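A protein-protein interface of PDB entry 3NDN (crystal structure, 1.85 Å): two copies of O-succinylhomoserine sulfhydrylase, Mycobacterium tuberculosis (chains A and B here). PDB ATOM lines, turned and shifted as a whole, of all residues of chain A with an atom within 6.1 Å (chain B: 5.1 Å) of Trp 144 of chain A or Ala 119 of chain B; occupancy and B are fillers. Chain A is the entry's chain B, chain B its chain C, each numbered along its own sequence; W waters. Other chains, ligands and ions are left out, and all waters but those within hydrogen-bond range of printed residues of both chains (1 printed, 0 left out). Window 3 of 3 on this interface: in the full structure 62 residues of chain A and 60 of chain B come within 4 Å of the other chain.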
ATOM      1  N   PHE A 110       8.111 -22.050   8.584  1.00  0.00           N
ATOM      2  CA  PHE A 110       9.462 -22.582   8.632  1.00  0.00           C
ATOM      3  C   PHE A 110      10.222 -22.554   7.290  1.00  0.00           C
ATOM      4  O   PHE A 110      11.387 -22.114   7.233  1.00  0.00           O
ATOM      5  CB  PHE A 110       9.499 -24.000   9.246  1.00  0.00           C
ATOM      6  CG  PHE A 110      10.865 -24.635   9.174  1.00  0.00           C
ATOM      7  CD1 PHE A 110      11.872 -24.237  10.056  1.00  0.00           C
ATOM      8  CD2 PHE A 110      11.159 -25.589   8.199  1.00  0.00           C
ATOM      9  CE1 PHE A 110      13.170 -24.789   9.971  1.00  0.00           C
ATOM     10  CE2 PHE A 110      12.442 -26.151   8.109  1.00  0.00           C
ATOM     11  CZ  PHE A 110      13.447 -25.743   8.999  1.00  0.00           C
ATOM     12  N   GLY A 118      20.503 -19.340   6.367  1.00  0.00           N
ATOM     13  CA  GLY A 118      21.433 -20.437   6.663  1.00  0.00           C
ATOM     14  C   GLY A 118      22.255 -20.120   7.909  1.00  0.00           C
ATOM     15  O   GLY A 118      22.082 -19.055   8.510  1.00  0.00           O
ATOM     16  N   ALA A 119      23.136 -21.043   8.309  1.00  0.00           N
ATOM     17  CA  ALA A 119      24.001 -20.822   9.472  1.00  0.00           C
ATOM     18  C   ALA A 119      24.839 -19.567   9.254  1.00  0.00           C
ATOM     19  O   ALA A 119      25.362 -19.351   8.156  1.00  0.00           O
ATOM     20  CB  ALA A 119      24.902 -22.051   9.744  1.00  0.00           C
ATOM     21  N   GLY A 120      24.936 -18.738  10.293  1.00  0.00           N
ATOM     22  CA  GLY A 120      25.640 -17.455  10.214  1.00  0.00           C
ATOM     23  C   GLY A 120      24.763 -16.255   9.880  1.00  0.00           C
ATOM     24  O   GLY A 120      25.195 -15.111  10.044  1.00  0.00           O
ATOM     25  N   GLU A 139      14.219 -21.180  19.022  1.00  0.00           N
ATOM     26  CA  GLU A 139      14.903 -22.439  19.343  1.00  0.00           C
ATOM     27  C   GLU A 139      15.364 -23.263  18.130  1.00  0.00           C
ATOM     28  O   GLU A 139      16.547 -23.654  18.037  1.00  0.00           O
ATOM     29  CB  GLU A 139      14.043 -23.288  20.298  1.00  0.00           C
ATOM     30  CG  GLU A 139      13.951 -22.694  21.706  1.00  0.00           C
ATOM     31  CD  GLU A 139      12.875 -23.333  22.578  1.00  0.00           C
ATOM     32  OE1 GLU A 139      12.462 -24.477  22.303  1.00  0.00           O
ATOM     33  OE2 GLU A 139      12.446 -22.686  23.557  1.00  0.00           O
ATOM     34  N   ILE A 140      14.440 -23.521  17.211  1.00  0.00           N
ATOM     35  CA  ILE A 140      14.703 -24.411  16.086  1.00  0.00           C
ATOM     36  C   ILE A 140      15.732 -23.857  15.079  1.00  0.00           C
ATOM     37  O   ILE A 140      16.697 -24.543  14.752  1.00  0.00           O
ATOM     38  CB  ILE A 140      13.390 -24.875  15.396  1.00  0.00           C
ATOM     39  CG1 ILE A 140      12.556 -25.724  16.371  1.00  0.00           C
ATOM     40  CG2 ILE A 140      13.694 -25.642  14.113  1.00  0.00           C
ATOM     41  CD1 ILE A 140      11.201 -26.217  15.801  1.00  0.00           C
ATOM     42  N   LEU A 141      15.539 -22.631  14.597  1.00  0.00           N
ATOM     43  CA  LEU A 141      16.516 -22.018  13.683  1.00  0.00           C
ATOM     44  C   LEU A 141      17.878 -21.665  14.332  1.00  0.00           C
ATOM     45  O   LEU A 141      18.922 -21.851  13.699  1.00  0.00           O
ATOM     46  CB  LEU A 141      15.904 -20.801  12.925  1.00  0.00           C
ATOM     47  CG  LEU A 141      14.927 -21.123  11.777  1.00  0.00           C
ATOM     48  CD1 LEU A 141      14.119 -19.884  11.369  1.00  0.00           C
ATOM     49  CD2 LEU A 141      15.632 -21.730  10.545  1.00  0.00           C
ATOM     50  N   PRO A 142      17.885 -21.158  15.583  1.00  0.00           N
ATOM     51  CA  PRO A 142      19.195 -20.970  16.239  1.00  0.00           C
ATOM     52  C   PRO A 142      20.001 -22.264  16.486  1.00  0.00           C
ATOM     53  O   PRO A 142      21.241 -22.211  16.505  1.00  0.00           O
ATOM     54  CB  PRO A 142      18.826 -20.293  17.568  1.00  0.00           C
ATOM     55  CG  PRO A 142      17.568 -19.533  17.247  1.00  0.00           C
ATOM     56  CD  PRO A 142      16.805 -20.494  16.344  1.00  0.00           C
ATOM     57  N   ARG A 143      19.323 -23.404  16.649  1.00  0.00           N
ATOM     58  CA  ARG A 143      20.007 -24.719  16.737  1.00  0.00           C
ATOM     59  C   ARG A 143      20.756 -25.046  15.427  1.00  0.00           C
ATOM     60  O   ARG A 143      21.750 -25.787  15.429  1.00  0.00           O
ATOM     61  CB  ARG A 143      19.029 -25.846  17.115  1.00  0.00           C
ATOM     62  CG  ARG A 143      19.651 -27.245  17.229  1.00  0.00           C
ATOM     63  CD  ARG A 143      18.655 -28.262  17.779  1.00  0.00           C
ATOM     64  NE  ARG A 143      19.086 -29.652  17.600  1.00  0.00           N
ATOM     65  CZ  ARG A 143      18.872 -30.392  16.505  1.00  0.00           C
ATOM     66  NH1 ARG A 143      18.262 -29.879  15.435  1.00  0.00           N
ATOM     67  NH2 ARG A 143      19.300 -31.651  16.467  1.00  0.00           N
ATOM     68  N   TRP A 144      20.296 -24.451  14.328  1.00  0.00           N
ATOM     69  CA  TRP A 144      20.935 -24.613  13.019  1.00  0.00           C
ATOM     70  C   TRP A 144      21.802 -23.385  12.652  1.00  0.00           C
ATOM     71  O   TRP A 144      22.068 -23.120  11.475  1.00  0.00           O
ATOM     72  CB  TRP A 144      19.888 -24.994  11.926  1.00  0.00           C
ATOM     73  CG  TRP A 144      19.443 -26.467  11.981  1.00  0.00           C
ATOM     74  CD1 TRP A 144      20.241 -27.548  12.257  1.00  0.00           C
ATOM     75  CD2 TRP A 144      18.119 -27.007  11.741  1.00  0.00           C
ATOM     76  NE1 TRP A 144      19.501 -28.711  12.219  1.00  0.00           N
ATOM     77  CE2 TRP A 144      18.201 -28.410  11.911  1.00  0.00           C
ATOM     78  CE3 TRP A 144      16.877 -26.440  11.419  1.00  0.00           C
ATOM     79  CZ2 TRP A 144      17.090 -29.256  11.759  1.00  0.00           C
ATOM     80  CZ3 TRP A 144      15.760 -27.289  11.270  1.00  0.00           C
ATOM     81  CH2 TRP A 144      15.877 -28.672  11.443  1.00  0.00           C
ATOM     82  N   GLY A 145      22.213 -22.626  13.674  1.00  0.00           N
ATOM     83  CA  GLY A 145      23.203 -21.542  13.518  1.00  0.00           C
ATOM     84  C   GLY A 145      22.724 -20.140  13.142  1.00  0.00           C
ATOM     85  O   GLY A 145      23.551 -19.267  12.809  1.00  0.00           O
ATOM     86  N   VAL A 146      21.405 -19.919  13.179  1.00  0.00           N
ATOM     87  CA  VAL A 146      20.821 -18.598  12.878  1.00  0.00           C
ATOM     88  C   VAL A 146      20.916 -17.716  14.134  1.00  0.00           C
ATOM     89  O   VAL A 146      20.799 -18.224  15.260  1.00  0.00           O
ATOM     90  CB  VAL A 146      19.327 -18.716  12.369  1.00  0.00           C
ATOM     91  CG1 VAL A 146      18.650 -17.338  12.229  1.00  0.00           C
ATOM     92  CG2 VAL A 146      19.274 -19.420  11.010  1.00  0.00           C
ATOM     93  N   PHE B 110      14.391 -36.225   6.048  1.00  0.00           N
ATOM     94  CA  PHE B 110      14.909 -34.957   6.579  1.00  0.00           C
ATOM     95  C   PHE B 110      14.665 -34.765   8.069  1.00  0.00           C
ATOM     96  O   PHE B 110      15.554 -34.302   8.801  1.00  0.00           O
ATOM     97  CB  PHE B 110      14.380 -33.714   5.807  1.00  0.00           C
ATOM     98  CG  PHE B 110      14.750 -32.410   6.469  1.00  0.00           C
ATOM     99  CD1 PHE B 110      16.077 -31.939   6.415  1.00  0.00           C
ATOM    100  CD2 PHE B 110      13.807 -31.685   7.201  1.00  0.00           C
ATOM    101  CE1 PHE B 110      16.446 -30.756   7.056  1.00  0.00           C
ATOM    102  CE2 PHE B 110      14.161 -30.495   7.847  1.00  0.00           C
ATOM    103  CZ  PHE B 110      15.486 -30.029   7.776  1.00  0.00           C
ATOM    104  N   GLY B 114      17.366 -34.454  11.003  1.00  0.00           N
ATOM    105  CA  GLY B 114      17.276 -33.170  11.693  1.00  0.00           C
ATOM    106  C   GLY B 114      17.123 -33.270  13.203  1.00  0.00           C
ATOM    107  O   GLY B 114      17.700 -32.462  13.950  1.00  0.00           O
ATOM    108  N   LEU B 117      20.801 -34.141  14.404  1.00  0.00           N
ATOM    109  CA  LEU B 117      21.916 -33.322  13.936  1.00  0.00           C
ATOM    110  C   LEU B 117      21.593 -31.832  13.971  1.00  0.00           C
ATOM    111  O   LEU B 117      20.731 -31.361  13.230  1.00  0.00           O
ATOM    112  CB  LEU B 117      22.304 -33.721  12.502  1.00  0.00           C
ATOM    113  CG  LEU B 117      22.687 -35.186  12.229  1.00  0.00           C
ATOM    114  CD1 LEU B 117      22.550 -35.518  10.754  1.00  0.00           C
ATOM    115  CD2 LEU B 117      24.104 -35.507  12.728  1.00  0.00           C
ATOM    116  N   GLY B 118      22.277 -31.103  14.854  1.00  0.00           N
ATOM    117  CA  GLY B 118      22.253 -29.642  14.853  1.00  0.00           C
ATOM    118  C   GLY B 118      23.589 -29.119  14.345  1.00  0.00           C
ATOM    119  O   GLY B 118      24.495 -29.906  14.041  1.00  0.00           O
ATOM    120  N   ALA B 119      23.720 -27.800  14.241  1.00  0.00           N
ATOM    121  CA  ALA B 119      24.982 -27.201  13.800  1.00  0.00           C
ATOM    122  C   ALA B 119      26.139 -27.683  14.697  1.00  0.00           C
ATOM    123  O   ALA B 119      26.024 -27.692  15.926  1.00  0.00           O
ATOM    124  CB  ALA B 119      24.879 -25.670  13.781  1.00  0.00           C
ATOM    125  N   GLY B 120      27.222 -28.137  14.066  1.00  0.00           N
ATOM    126  CA  GLY B 120      28.401 -28.639  14.789  1.00  0.00           C
ATOM    127  C   GLY B 120      28.441 -30.143  14.987  1.00  0.00           C
ATOM    128  O   GLY B 120      29.387 -30.668  15.578  1.00  0.00           O
ATOM    129  N   ASP B 121      27.422 -30.846  14.488  1.00  0.00           N
ATOM    130  CA  ASP B 121      27.346 -32.303  14.621  1.00  0.00           C
ATOM    131  C   ASP B 121      27.816 -33.005  13.339  1.00  0.00           C
ATOM    132  O   ASP B 121      27.950 -32.376  12.288  1.00  0.00           O
ATOM    133  CB  ASP B 121      25.922 -32.744  15.009  1.00  0.00           C
ATOM    134  CG  ASP B 121      25.522 -32.290  16.413  1.00  0.00           C
ATOM    135  OD1 ASP B 121      26.412 -32.088  17.275  1.00  0.00           O
ATOM    136  OD2 ASP B 121      24.303 -32.147  16.668  1.00  0.00           O
ATOM    137  N   LEU B 141      21.562 -30.039   4.783  1.00  0.00           N
ATOM    138  CA  LEU B 141      22.009 -30.079   6.175  1.00  0.00           C
ATOM    139  C   LEU B 141      23.383 -29.372   6.403  1.00  0.00           C
ATOM    140  O   LEU B 141      23.555 -28.682   7.412  1.00  0.00           O
ATOM    141  CB  LEU B 141      21.985 -31.515   6.729  1.00  0.00           C
ATOM    142  CG  LEU B 141      20.625 -32.178   7.025  1.00  0.00           C
ATOM    143  CD1 LEU B 141      20.798 -33.691   7.118  1.00  0.00           C
ATOM    144  CD2 LEU B 141      20.009 -31.647   8.314  1.00  0.00           C
ATOM    145  N   TRP B 144      23.109 -25.729   7.098  1.00  0.00           N
ATOM    146  CA  TRP B 144      22.739 -25.477   8.488  1.00  0.00           C
ATOM    147  C   TRP B 144      23.791 -26.030   9.481  1.00  0.00           C
ATOM    148  O   TRP B 144      23.501 -26.275  10.661  1.00  0.00           O
ATOM    149  CB  TRP B 144      21.331 -26.030   8.776  1.00  0.00           C
ATOM    150  CG  TRP B 144      20.209 -25.141   8.279  1.00  0.00           C
ATOM    151  CD1 TRP B 144      20.143 -23.777   8.364  1.00  0.00           C
ATOM    152  CD2 TRP B 144      18.983 -25.565   7.644  1.00  0.00           C
ATOM    153  NE1 TRP B 144      18.960 -23.319   7.797  1.00  0.00           N
ATOM    154  CE2 TRP B 144      18.239 -24.395   7.343  1.00  0.00           C
ATOM    155  CE3 TRP B 144      18.461 -26.813   7.269  1.00  0.00           C
ATOM    156  CZ2 TRP B 144      16.976 -24.440   6.712  1.00  0.00           C
ATOM    157  CZ3 TRP B 144      17.206 -26.861   6.636  1.00  0.00           C
ATOM    158  CH2 TRP B 144      16.485 -25.673   6.359  1.00  0.00           C
ATOM    159  N   GLY B 145      25.012 -26.221   8.985  1.00  0.00           N
ATOM    160  CA  GLY B 145      26.173 -26.384   9.859  1.00  0.00           C
ATOM    161  C   GLY B 145      26.612 -27.797  10.190  1.00  0.00           C
ATOM    162  O   GLY B 145      27.539 -27.984  10.977  1.00  0.00           O
ATOM    163  N   VAL B 146      25.957 -28.785   9.582  1.00  0.00           N
ATOM    164  CA  VAL B 146      26.298 -30.191   9.767  1.00  0.00           C
ATOM    165  C   VAL B 146      27.532 -30.581   8.928  1.00  0.00           C
ATOM    166  O   VAL B 146      27.684 -30.155   7.775  1.00  0.00           O
ATOM    167  CB  VAL B 146      25.084 -31.118   9.447  1.00  0.00           C
ATOM    168  CG1 VAL B 146      25.474 -32.584   9.515  1.00  0.00           C
ATOM    169  CG2 VAL B 146      23.919 -30.853  10.426  1.00  0.00           C
ATOM    170  N   LEU B 254      10.098 -31.234  16.328  1.00  0.00           N
ATOM    171  CA  LEU B 254      10.159 -30.804  14.930  1.00  0.00           C
ATOM    172  C   LEU B 254       8.814 -30.971  14.206  1.00  0.00           C
ATOM    173  O   LEU B 254       8.406 -30.098  13.414  1.00  0.00           O
ATOM    174  CB  LEU B 254      11.281 -31.538  14.184  1.00  0.00           C
ATOM    175  CG  LEU B 254      12.718 -31.104  14.519  1.00  0.00           C
ATOM    176  CD1 LEU B 254      13.712 -31.892  13.671  1.00  0.00           C
ATOM    177  CD2 LEU B 254      12.890 -29.602  14.275  1.00  0.00           C
HETATM  178  O   HOH W   1      23.738 -26.202  17.556  1.00  0.00           O
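Water W1 lies within hydrogen-bond range of the backbone carbonyl oxygen of Arg 143 of chain A (2.9 Å) and the backbone carbonyl oxygen of Ala 119 of chain B (3.2 Å).
Of the printed residues of chain B, Trp 144 of chain A touches Phe 110, Gly 114, Leu 117, Gly 118, Ala 119 and Trp 144. Of the printed residues of chain A, Ala 119 of chain B touches Arg 143 and Trp 144. Of the printed residues of chain A, Phe 110 of chain B touches Trp 144 (3.9 Å). Of the printed residues of chain A, Gly 118 of chain B touches Arg 143 (3.4 Å) and Trp 144 (3.9 Å). Printed residues of chain B within 4 Å of Arg 143 of chain A: Gly 114 (3.0 Å), Leu 117 (3.4 Å), Gly 118 (3.4 Å) and Ala 119 (3.1 Å). Printed residues of chain A within 4 Å of Trp 144 of chain B: Gly 118 and Trp 144. Gly 120 of chain A touches none of the printed residues of chain B. The nearest printed residue of chain B that does not touch Trp 144 of chain A is Leu 254 of chain B (4.2 Å). The nearest printed residue of chain A that does not touch Ala 119 of chain B is Gly 145 of chain A (4.05 Å). The nearest printed residue of chain A that does not touch Leu 117 of chain B is Ile 140 of chain A (8.1 Å).
N of Gly 118 of chain B lies within hydrogen-bond range of OD2 of Asp 121 of chain B, at 2.9 Å.
Gly 118 of chain A touches Trp 144 of chain B, and with the chains exchanged Trp 144 of chain A touches Gly 118 of chain B. Trp 144 of chain A touches Phe 110 of chain B, but with the chains exchanged Phe 110 of chain A does not touch Trp 144 of chain B (4.03 Å). Trp 144 of chain A touches Ala 119 of chain B, but with the chains exchanged Ala 119 of chain A does not touch Trp 144 of chain B (4.1 Å). Trp 144 of chain A touches its own counterpart, Trp 144 of chain B. Of the 11 pairs that touch across the chains among the printed residues, 3 have their exchanged pair printed and touching as well.
Among the printed residues, pairs that only touch across the chains: Arg 143 of chain A with Leu 117 of chain B, Trp 144 of chain A with Trp 144 of chain B, Trp 144 of chain A with Gly 118 of chain B, Trp 144 of chain A with Gly 114 of chain B, Trp 144 of chain A with Phe 110 of chain B, Gly 118 of chain A with Trp 144 of chain B and Trp 144 of chain A with Ala 119 of chain B.
The backbone carbonyl oxygen of Arg 143 of chain A sits at hydrogen-bond distance from the backbone NH of Ala 119 of chain B, 3.1 Å away. The guanidinium group of Arg 143 of chain A lies within hydrogen-bond range of the backbone carbonyl oxygen of Gly 114 of chain B (3.0 Å). The indole nitrogen of Trp 144 of chain A lies within hydrogen-bond range of the backbone carbonyl oxygen of Leu 117 of chain B (3.1 Å). The guanidinium group of Arg 143 of chain A sits close to the backbone NH of Gly 118 of chain B (3.4 Å).
Printed residues of chain B that touch a printed residue of chain A: Phe 110, Gly 114, Leu 117, Gly 118, Ala 119 and Trp 144. Hydrophobic or aromatic side chains of chain B that line the printed part of chain A: Phe 110, Ala 119 and Trp 144. Hydrophobic or aromatic side chains of chain A within 4 Å of the printed part of chain B: Trp 144. Among the printed residues, no Asp or Glu carboxylate lies within 4 Å of a Lys or Arg side-chain nitrogen of the other chain.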
